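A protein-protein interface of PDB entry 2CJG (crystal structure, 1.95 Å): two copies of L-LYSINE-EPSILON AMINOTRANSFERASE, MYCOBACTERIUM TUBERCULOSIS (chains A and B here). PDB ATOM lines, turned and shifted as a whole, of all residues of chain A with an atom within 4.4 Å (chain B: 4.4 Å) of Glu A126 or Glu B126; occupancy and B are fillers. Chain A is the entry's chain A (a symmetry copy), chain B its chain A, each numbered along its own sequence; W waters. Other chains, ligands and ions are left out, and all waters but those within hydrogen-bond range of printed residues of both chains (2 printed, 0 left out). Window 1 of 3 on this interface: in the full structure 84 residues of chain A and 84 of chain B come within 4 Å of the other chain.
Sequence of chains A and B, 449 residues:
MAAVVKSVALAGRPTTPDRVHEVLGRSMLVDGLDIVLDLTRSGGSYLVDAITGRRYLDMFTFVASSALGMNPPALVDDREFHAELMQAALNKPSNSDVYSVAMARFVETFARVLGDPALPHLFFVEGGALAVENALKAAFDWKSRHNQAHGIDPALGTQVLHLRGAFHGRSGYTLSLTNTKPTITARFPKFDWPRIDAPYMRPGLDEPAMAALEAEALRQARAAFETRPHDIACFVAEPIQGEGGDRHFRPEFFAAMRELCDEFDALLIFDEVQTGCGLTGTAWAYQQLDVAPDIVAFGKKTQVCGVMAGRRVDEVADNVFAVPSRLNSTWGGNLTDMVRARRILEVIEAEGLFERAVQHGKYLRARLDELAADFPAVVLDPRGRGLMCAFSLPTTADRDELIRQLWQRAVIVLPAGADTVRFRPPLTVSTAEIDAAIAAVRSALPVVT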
ATOM      1  N   LYS A  92      -1.909   2.266 -18.183  1.00  0.00           N
ATOM      2  CA  LYS A  92      -3.071   1.605 -18.797  1.00  0.00           C
ATOM      3  C   LYS A  92      -3.326   2.318 -20.117  1.00  0.00           C
ATOM      4  O   LYS A  92      -4.096   3.269 -20.176  1.00  0.00           O
ATOM      5  CB  LYS A  92      -4.304   1.593 -17.865  1.00  0.00           C
ATOM      6  CG  LYS A  92      -5.470   0.724 -18.354  1.00  0.00           C
ATOM      7  CD  LYS A  92      -6.708   0.823 -17.467  1.00  0.00           C
ATOM      8  CE  LYS A  92      -7.782  -0.129 -17.986  1.00  0.00           C
ATOM      9  NZ  LYS A  92      -9.014  -0.127 -17.141  1.00  0.00           N
ATOM     10  N   VAL A 125     -12.406  -5.992 -25.600  1.00  0.00           N
ATOM     11  CA  VAL A 125     -13.112  -5.031 -24.793  1.00  0.00           C
ATOM     12  C   VAL A 125     -13.004  -5.552 -23.322  1.00  0.00           C
ATOM     13  O   VAL A 125     -12.733  -6.755 -23.080  1.00  0.00           O
ATOM     14  CB  VAL A 125     -14.582  -4.898 -25.301  1.00  0.00           C
ATOM     15  CG1 VAL A 125     -15.370  -6.178 -25.042  1.00  0.00           C
ATOM     16  CG2 VAL A 125     -15.308  -3.707 -24.644  1.00  0.00           C
ATOM     17  N   GLU A 126     -13.177  -4.664 -22.354  1.00  0.00           N
ATOM     18  CA  GLU A 126     -13.265  -5.113 -20.955  1.00  0.00           C
ATOM     19  C   GLU A 126     -14.699  -5.564 -20.708  1.00  0.00           C
ATOM     20  O   GLU A 126     -15.618  -4.796 -20.978  1.00  0.00           O
ATOM     21  CB  GLU A 126     -12.965  -3.951 -20.004  1.00  0.00           C
ATOM     22  CG  GLU A 126     -11.486  -3.493 -19.993  1.00  0.00           C
ATOM     23  CD  GLU A 126     -11.242  -2.363 -18.942  1.00  0.00           C
ATOM     24  OE1 GLU A 126     -12.136  -1.498 -18.728  1.00  0.00           O
ATOM     25  OE2 GLU A 126     -10.163  -2.356 -18.345  1.00  0.00           O
ATOM     26  N   GLY A 127     -14.884  -6.782 -20.202  1.00  0.00           N
ATOM     27  CA  GLY A 127     -16.181  -7.197 -19.640  1.00  0.00           C
ATOM     28  C   GLY A 127     -16.936  -8.179 -20.542  1.00  0.00           C
ATOM     29  O   GLY A 127     -16.999  -7.965 -21.758  1.00  0.00           O
ATOM     30  N   LEU A 130     -20.229  -6.792 -22.379  1.00  0.00           N
ATOM     31  CA  LEU A 130     -19.866  -5.942 -23.512  1.00  0.00           C
ATOM     32  C   LEU A 130     -19.325  -6.767 -24.697  1.00  0.00           C
ATOM     33  O   LEU A 130     -19.525  -6.406 -25.840  1.00  0.00           O
ATOM     34  CB  LEU A 130     -18.864  -4.859 -23.091  1.00  0.00           C
ATOM     35  CG  LEU A 130     -19.441  -3.433 -23.221  1.00  0.00           C
ATOM     36  CD1 LEU A 130     -20.850  -3.349 -22.695  1.00  0.00           C
ATOM     37  CD2 LEU A 130     -18.546  -2.413 -22.543  1.00  0.00           C
ATOM     38  N   TRP A 331     -10.388   2.034 -23.821  1.00  0.00           N
ATOM     39  CA  TRP A 331      -9.148   1.269 -23.599  1.00  0.00           C
ATOM     40  C   TRP A 331      -8.868   0.138 -24.589  1.00  0.00           C
ATOM     41  O   TRP A 331      -7.696  -0.201 -24.807  1.00  0.00           O
ATOM     42  CB  TRP A 331      -9.083   0.728 -22.168  1.00  0.00           C
ATOM     43  CG  TRP A 331      -8.762   1.828 -21.134  1.00  0.00           C
ATOM     44  CD1 TRP A 331      -7.659   2.649 -21.103  1.00  0.00           C
ATOM     45  CD2 TRP A 331      -9.556   2.163 -19.972  1.00  0.00           C
ATOM     46  NE1 TRP A 331      -7.733   3.491 -19.989  1.00  0.00           N
ATOM     47  CE2 TRP A 331      -8.879   3.205 -19.284  1.00  0.00           C
ATOM     48  CE3 TRP A 331     -10.763   1.669 -19.446  1.00  0.00           C
ATOM     49  CZ2 TRP A 331      -9.385   3.778 -18.091  1.00  0.00           C
ATOM     50  CZ3 TRP A 331     -11.259   2.234 -18.260  1.00  0.00           C
ATOM     51  CH2 TRP A 331     -10.563   3.273 -17.596  1.00  0.00           C
ATOM     52  N   GLY A 333      -9.690  -3.009 -24.104  1.00  0.00           N
ATOM     53  CA  GLY A 333      -9.226  -4.115 -23.271  1.00  0.00           C
ATOM     54  C   GLY A 333      -8.081  -3.639 -22.392  1.00  0.00           C
ATOM     55  O   GLY A 333      -7.470  -2.583 -22.641  1.00  0.00           O
ATOM     56  N   ASN A 334      -7.799  -4.397 -21.361  1.00  0.00           N
ATOM     57  CA  ASN A 334      -6.823  -4.003 -20.373  1.00  0.00           C
ATOM     58  C   ASN A 334      -5.469  -4.639 -20.751  1.00  0.00           C
ATOM     59  O   ASN A 334      -5.355  -5.870 -20.899  1.00  0.00           O
ATOM     60  CB  ASN A 334      -7.314  -4.460 -19.001  1.00  0.00           C
ATOM     61  CG  ASN A 334      -6.532  -3.861 -17.861  1.00  0.00           C
ATOM     62  OD1 ASN A 334      -5.307  -3.928 -17.835  1.00  0.00           O
ATOM     63  ND2 ASN A 334      -7.242  -3.256 -16.901  1.00  0.00           N
ATOM     64  N   ASP A 337      -4.207  -7.458 -18.523  1.00  0.00           N
ATOM     65  CA  ASP A 337      -4.948  -8.694 -18.821  1.00  0.00           C
ATOM     66  C   ASP A 337      -4.449  -9.399 -20.093  1.00  0.00           C
ATOM     67  O   ASP A 337      -4.399 -10.628 -20.125  1.00  0.00           O
ATOM     68  CB  ASP A 337      -6.458  -8.391 -18.979  1.00  0.00           C
ATOM     69  CG  ASP A 337      -7.125  -8.090 -17.641  1.00  0.00           C
ATOM     70  OD1 ASP A 337      -6.537  -8.377 -16.590  1.00  0.00           O
ATOM     71  OD2 ASP A 337      -8.219  -7.569 -17.654  1.00  0.00           O
ATOM     72  N   LYS B  92      -6.531 -12.402 -11.200  1.00  0.00           N
ATOM     73  CA  LYS B  92      -7.615 -11.430 -11.417  1.00  0.00           C
ATOM     74  C   LYS B  92      -8.818 -11.941 -10.638  1.00  0.00           C
ATOM     75  O   LYS B  92      -9.645 -12.670 -11.171  1.00  0.00           O
ATOM     76  CB  LYS B  92      -7.913 -11.206 -12.917  1.00  0.00           C
ATOM     77  CG  LYS B  92      -8.868 -10.042 -13.215  1.00  0.00           C
ATOM     78  CD  LYS B  92      -9.226  -9.920 -14.693  1.00  0.00           C
ATOM     79  CE  LYS B  92     -10.113  -8.696 -14.901  1.00  0.00           C
ATOM     80  NZ  LYS B  92     -10.470  -8.477 -16.337  1.00  0.00           N
ATOM     81  N   VAL B 125     -16.961  -1.243 -11.543  1.00  0.00           N
ATOM     82  CA  VAL B 125     -17.189  -2.074 -12.696  1.00  0.00           C
ATOM     83  C   VAL B 125     -16.041  -1.727 -13.701  1.00  0.00           C
ATOM     84  O   VAL B 125     -15.400  -0.651 -13.606  1.00  0.00           O
ATOM     85  CB  VAL B 125     -18.618  -1.806 -13.264  1.00  0.00           C
ATOM     86  CG1 VAL B 125     -18.719  -0.403 -13.852  1.00  0.00           C
ATOM     87  CG2 VAL B 125     -19.011  -2.841 -14.335  1.00  0.00           C
ATOM     88  N   GLU B 126     -15.760  -2.631 -14.629  1.00  0.00           N
ATOM     89  CA  GLU B 126     -14.820  -2.300 -15.712  1.00  0.00           C
ATOM     90  C   GLU B 126     -15.598  -1.542 -16.779  1.00  0.00           C
ATOM     91  O   GLU B 126     -16.626  -2.041 -17.231  1.00  0.00           O
ATOM     92  CB  GLU B 126     -14.269  -3.579 -16.347  1.00  0.00           C
ATOM     93  CG  GLU B 126     -13.294  -4.378 -15.449  1.00  0.00           C
ATOM     94  CD  GLU B 126     -12.714  -5.622 -16.193  1.00  0.00           C
ATOM     95  OE1 GLU B 126     -13.435  -6.263 -17.007  1.00  0.00           O
ATOM     96  OE2 GLU B 126     -11.546  -5.941 -15.957  1.00  0.00           O
ATOM     97  N   GLY B 127     -15.117  -0.365 -17.176  1.00  0.00           N
ATOM     98  CA  GLY B 127     -15.602   0.297 -18.399  1.00  0.00           C
ATOM     99  C   GLY B 127     -16.496   1.507 -18.108  1.00  0.00           C
ATOM    100  O   GLY B 127     -17.373   1.424 -17.241  1.00  0.00           O
ATOM    101  N   LEU B 130     -20.406   1.119 -18.942  1.00  0.00           N
ATOM    102  CA  LEU B 130     -21.073   0.311 -17.922  1.00  0.00           C
ATOM    103  C   LEU B 130     -21.239   1.084 -16.599  1.00  0.00           C
ATOM    104  O   LEU B 130     -22.205   0.885 -15.887  1.00  0.00           O
ATOM    105  CB  LEU B 130     -20.332  -1.014 -17.696  1.00  0.00           C
ATOM    106  CG  LEU B 130     -21.177  -2.242 -18.094  1.00  0.00           C
ATOM    107  CD1 LEU B 130     -21.888  -2.032 -19.406  1.00  0.00           C
ATOM    108  CD2 LEU B 130     -20.335  -3.504 -18.127  1.00  0.00           C
ATOM    109  N   TRP B 331     -16.272  -9.644 -12.319  1.00  0.00           N
ATOM    110  CA  TRP B 331     -15.044  -9.222 -11.625  1.00  0.00           C
ATOM    111  C   TRP B 331     -15.202  -8.107 -10.589  1.00  0.00           C
ATOM    112  O   TRP B 331     -14.407  -8.041  -9.642  1.00  0.00           O
ATOM    113  CB  TRP B 331     -13.949  -8.841 -12.625  1.00  0.00           C
ATOM    114  CG  TRP B 331     -13.315 -10.074 -13.305  1.00  0.00           C
ATOM    115  CD1 TRP B 331     -12.687 -11.134 -12.695  1.00  0.00           C
ATOM    116  CD2 TRP B 331     -13.230 -10.311 -14.730  1.00  0.00           C
ATOM    117  NE1 TRP B 331     -12.230 -12.029 -13.665  1.00  0.00           N
ATOM    118  CE2 TRP B 331     -12.544 -11.541 -14.913  1.00  0.00           C
ATOM    119  CE3 TRP B 331     -13.653  -9.590 -15.861  1.00  0.00           C
ATOM    120  CZ2 TRP B 331     -12.286 -12.080 -16.197  1.00  0.00           C
ATOM    121  CZ3 TRP B 331     -13.391 -10.123 -17.133  1.00  0.00           C
ATOM    122  CH2 TRP B 331     -12.705 -11.353 -17.285  1.00  0.00           C
ATOM    123  N   GLY B 333     -14.736  -4.911 -11.206  1.00  0.00           N
ATOM    124  CA  GLY B 333     -13.599  -4.027 -11.445  1.00  0.00           C
ATOM    125  C   GLY B 333     -12.316  -4.840 -11.423  1.00  0.00           C
ATOM    126  O   GLY B 333     -12.282  -5.985 -10.936  1.00  0.00           O
ATOM    127  N   ASN B 334     -11.267  -4.266 -11.961  1.00  0.00           N
ATOM    128  CA  ASN B 334     -10.017  -4.969 -12.124  1.00  0.00           C
ATOM    129  C   ASN B 334      -9.119  -4.645 -10.911  1.00  0.00           C
ATOM    130  O   ASN B 334      -8.836  -3.469 -10.616  1.00  0.00           O
ATOM    131  CB  ASN B 334      -9.385  -4.531 -13.443  1.00  0.00           C
ATOM    132  CG  ASN B 334      -8.228  -5.399 -13.864  1.00  0.00           C
ATOM    133  OD1 ASN B 334      -7.302  -5.630 -13.093  1.00  0.00           O
ATOM    134  ND2 ASN B 334      -8.274  -5.899 -15.105  1.00  0.00           N
ATOM    135  N   ASP B 337      -6.095  -2.419 -11.550  1.00  0.00           N
ATOM    136  CA  ASP B 337      -6.530  -1.021 -11.687  1.00  0.00           C
ATOM    137  C   ASP B 337      -6.812  -0.345 -10.336  1.00  0.00           C
ATOM    138  O   ASP B 337      -6.502   0.833 -10.169  1.00  0.00           O
ATOM    139  CB  ASP B 337      -7.804  -0.938 -12.562  1.00  0.00           C
ATOM    140  CG  ASP B 337      -7.505  -1.188 -14.037  1.00  0.00           C
ATOM    141  OD1 ASP B 337      -6.334  -1.145 -14.435  1.00  0.00           O
ATOM    142  OD2 ASP B 337      -8.436  -1.428 -14.774  1.00  0.00           O
HETATM  143  O   HOH W   1     -11.937  -7.581 -19.076  1.00  0.00           O
HETATM  144  O   HOH W   2     -12.055  -0.400 -16.073  1.00  0.00           O
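The side-chain amino group (NZ) of Lys B92 is in salt-bridge range of the side-chain carboxylate (OD2) of Asp A337. The side-chain amide nitrogen (ND2) of Asn A334 lies close to the side-chain amide nitrogen (ND2) of Asn B334, 3.4 Å away. ND2 of Asn B334 sits at hydrogen-bond distance from OD2 of Asp A337, at 3.0 Å. The side-chain carboxylate (OD2) of Asp B337 is in salt-bridge range of the side-chain amino group (NZ) of Lys A92 (2.8 Å). OD2 of Asp B337 is in hydrogen-bond range of ND2 of Asn A334 (3.0 Å).
The side-chain carboxylate (OE2) of Glu B126 is in salt-bridge range of the side-chain amino group (NZ) of Lys B92, at 2.8 Å. The side-chain amide nitrogen (ND2) of Asn B334 lies within hydrogen-bond range of the side-chain carboxylate (OE2) of Glu B126 (3.4 Å). The side-chain amino group (NZ) of Lys A92 is in salt-bridge range of the side-chain carboxylate (OE2) of Glu A126 (2.8 Å). OE2 of Glu A126 sits at hydrogen-bond distance from ND2 of Asn A334, at 3.4 Å.
Glu B126 touches Glu A126. Gly B127 touches Glu A126 (N to OE1, 3.5 Å). N of Gly A127 touches OE1 of Glu B126, at 3.5 Å. Leu B130 touches Leu A130.
Of chain B, only Glu B126 and Gly B127 come within 4 Å of Glu A126. Printed residues of chain B within 4 Å of Gly A127: Glu B126 (3.5 Å). Of the printed residues of chain B, Asn A334 touches Asn B334 and Asp B337. Of the printed residues of chain A, Lys B92 touches Asp A337. Printed residues of chain A within 4 Å of Leu B130: Leu A130 (3.7 Å). Trp B331 touches none of the printed residues of chain A. The nearest residue of chain A that does not touch Glu B126 is Asp A337 (4.1 Å). The nearest printed residue of chain A that does not touch Asn B334 is Glu A126 (5.2 Å).
Printed residues of chain B that touch a printed residue of chain A: Lys B92, Glu B126, Gly B127, Leu B130, Asn B334 and Asp B337. Hydrophobic or aromatic side chains of chain B that line the printed part of chain A: Leu B130. Of the 9 printed residues of chain A, 6 touch a printed residue of chain B. Hydrophobic or aromatic side chains of chain A that line the printed part of chain B: Leu A130.
Lys A92 touches Asp B337, and with the chains exchanged Asp A337 touches Lys B92. Glu B126 touches its own counterpart, Glu A126. Glu A126 touches Gly B127, and with the chains exchanged Gly A127 touches Glu B126. Asn B334 touches its own counterpart, Asn A334. Positions printed for both chains: 92, 125, 126, 127, 130, 331, 333, 334 and 337. Of the 9 pairs that touch across the chains among the printed residues, 9 have their exchanged pair printed and touching as well.
Water W1 lies within hydrogen-bond range of OE1 of Glu B126 (2.9 Å), NZ of Lys B92 (3.2 Å) and N of Gly A127 (3.3 Å). Water W2 lies within hydrogen-bond range of OE1 of Glu A126 (2.9 Å), NZ of Lys A92 (3.2 Å) and N of Gly B127 (3.3 Å).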
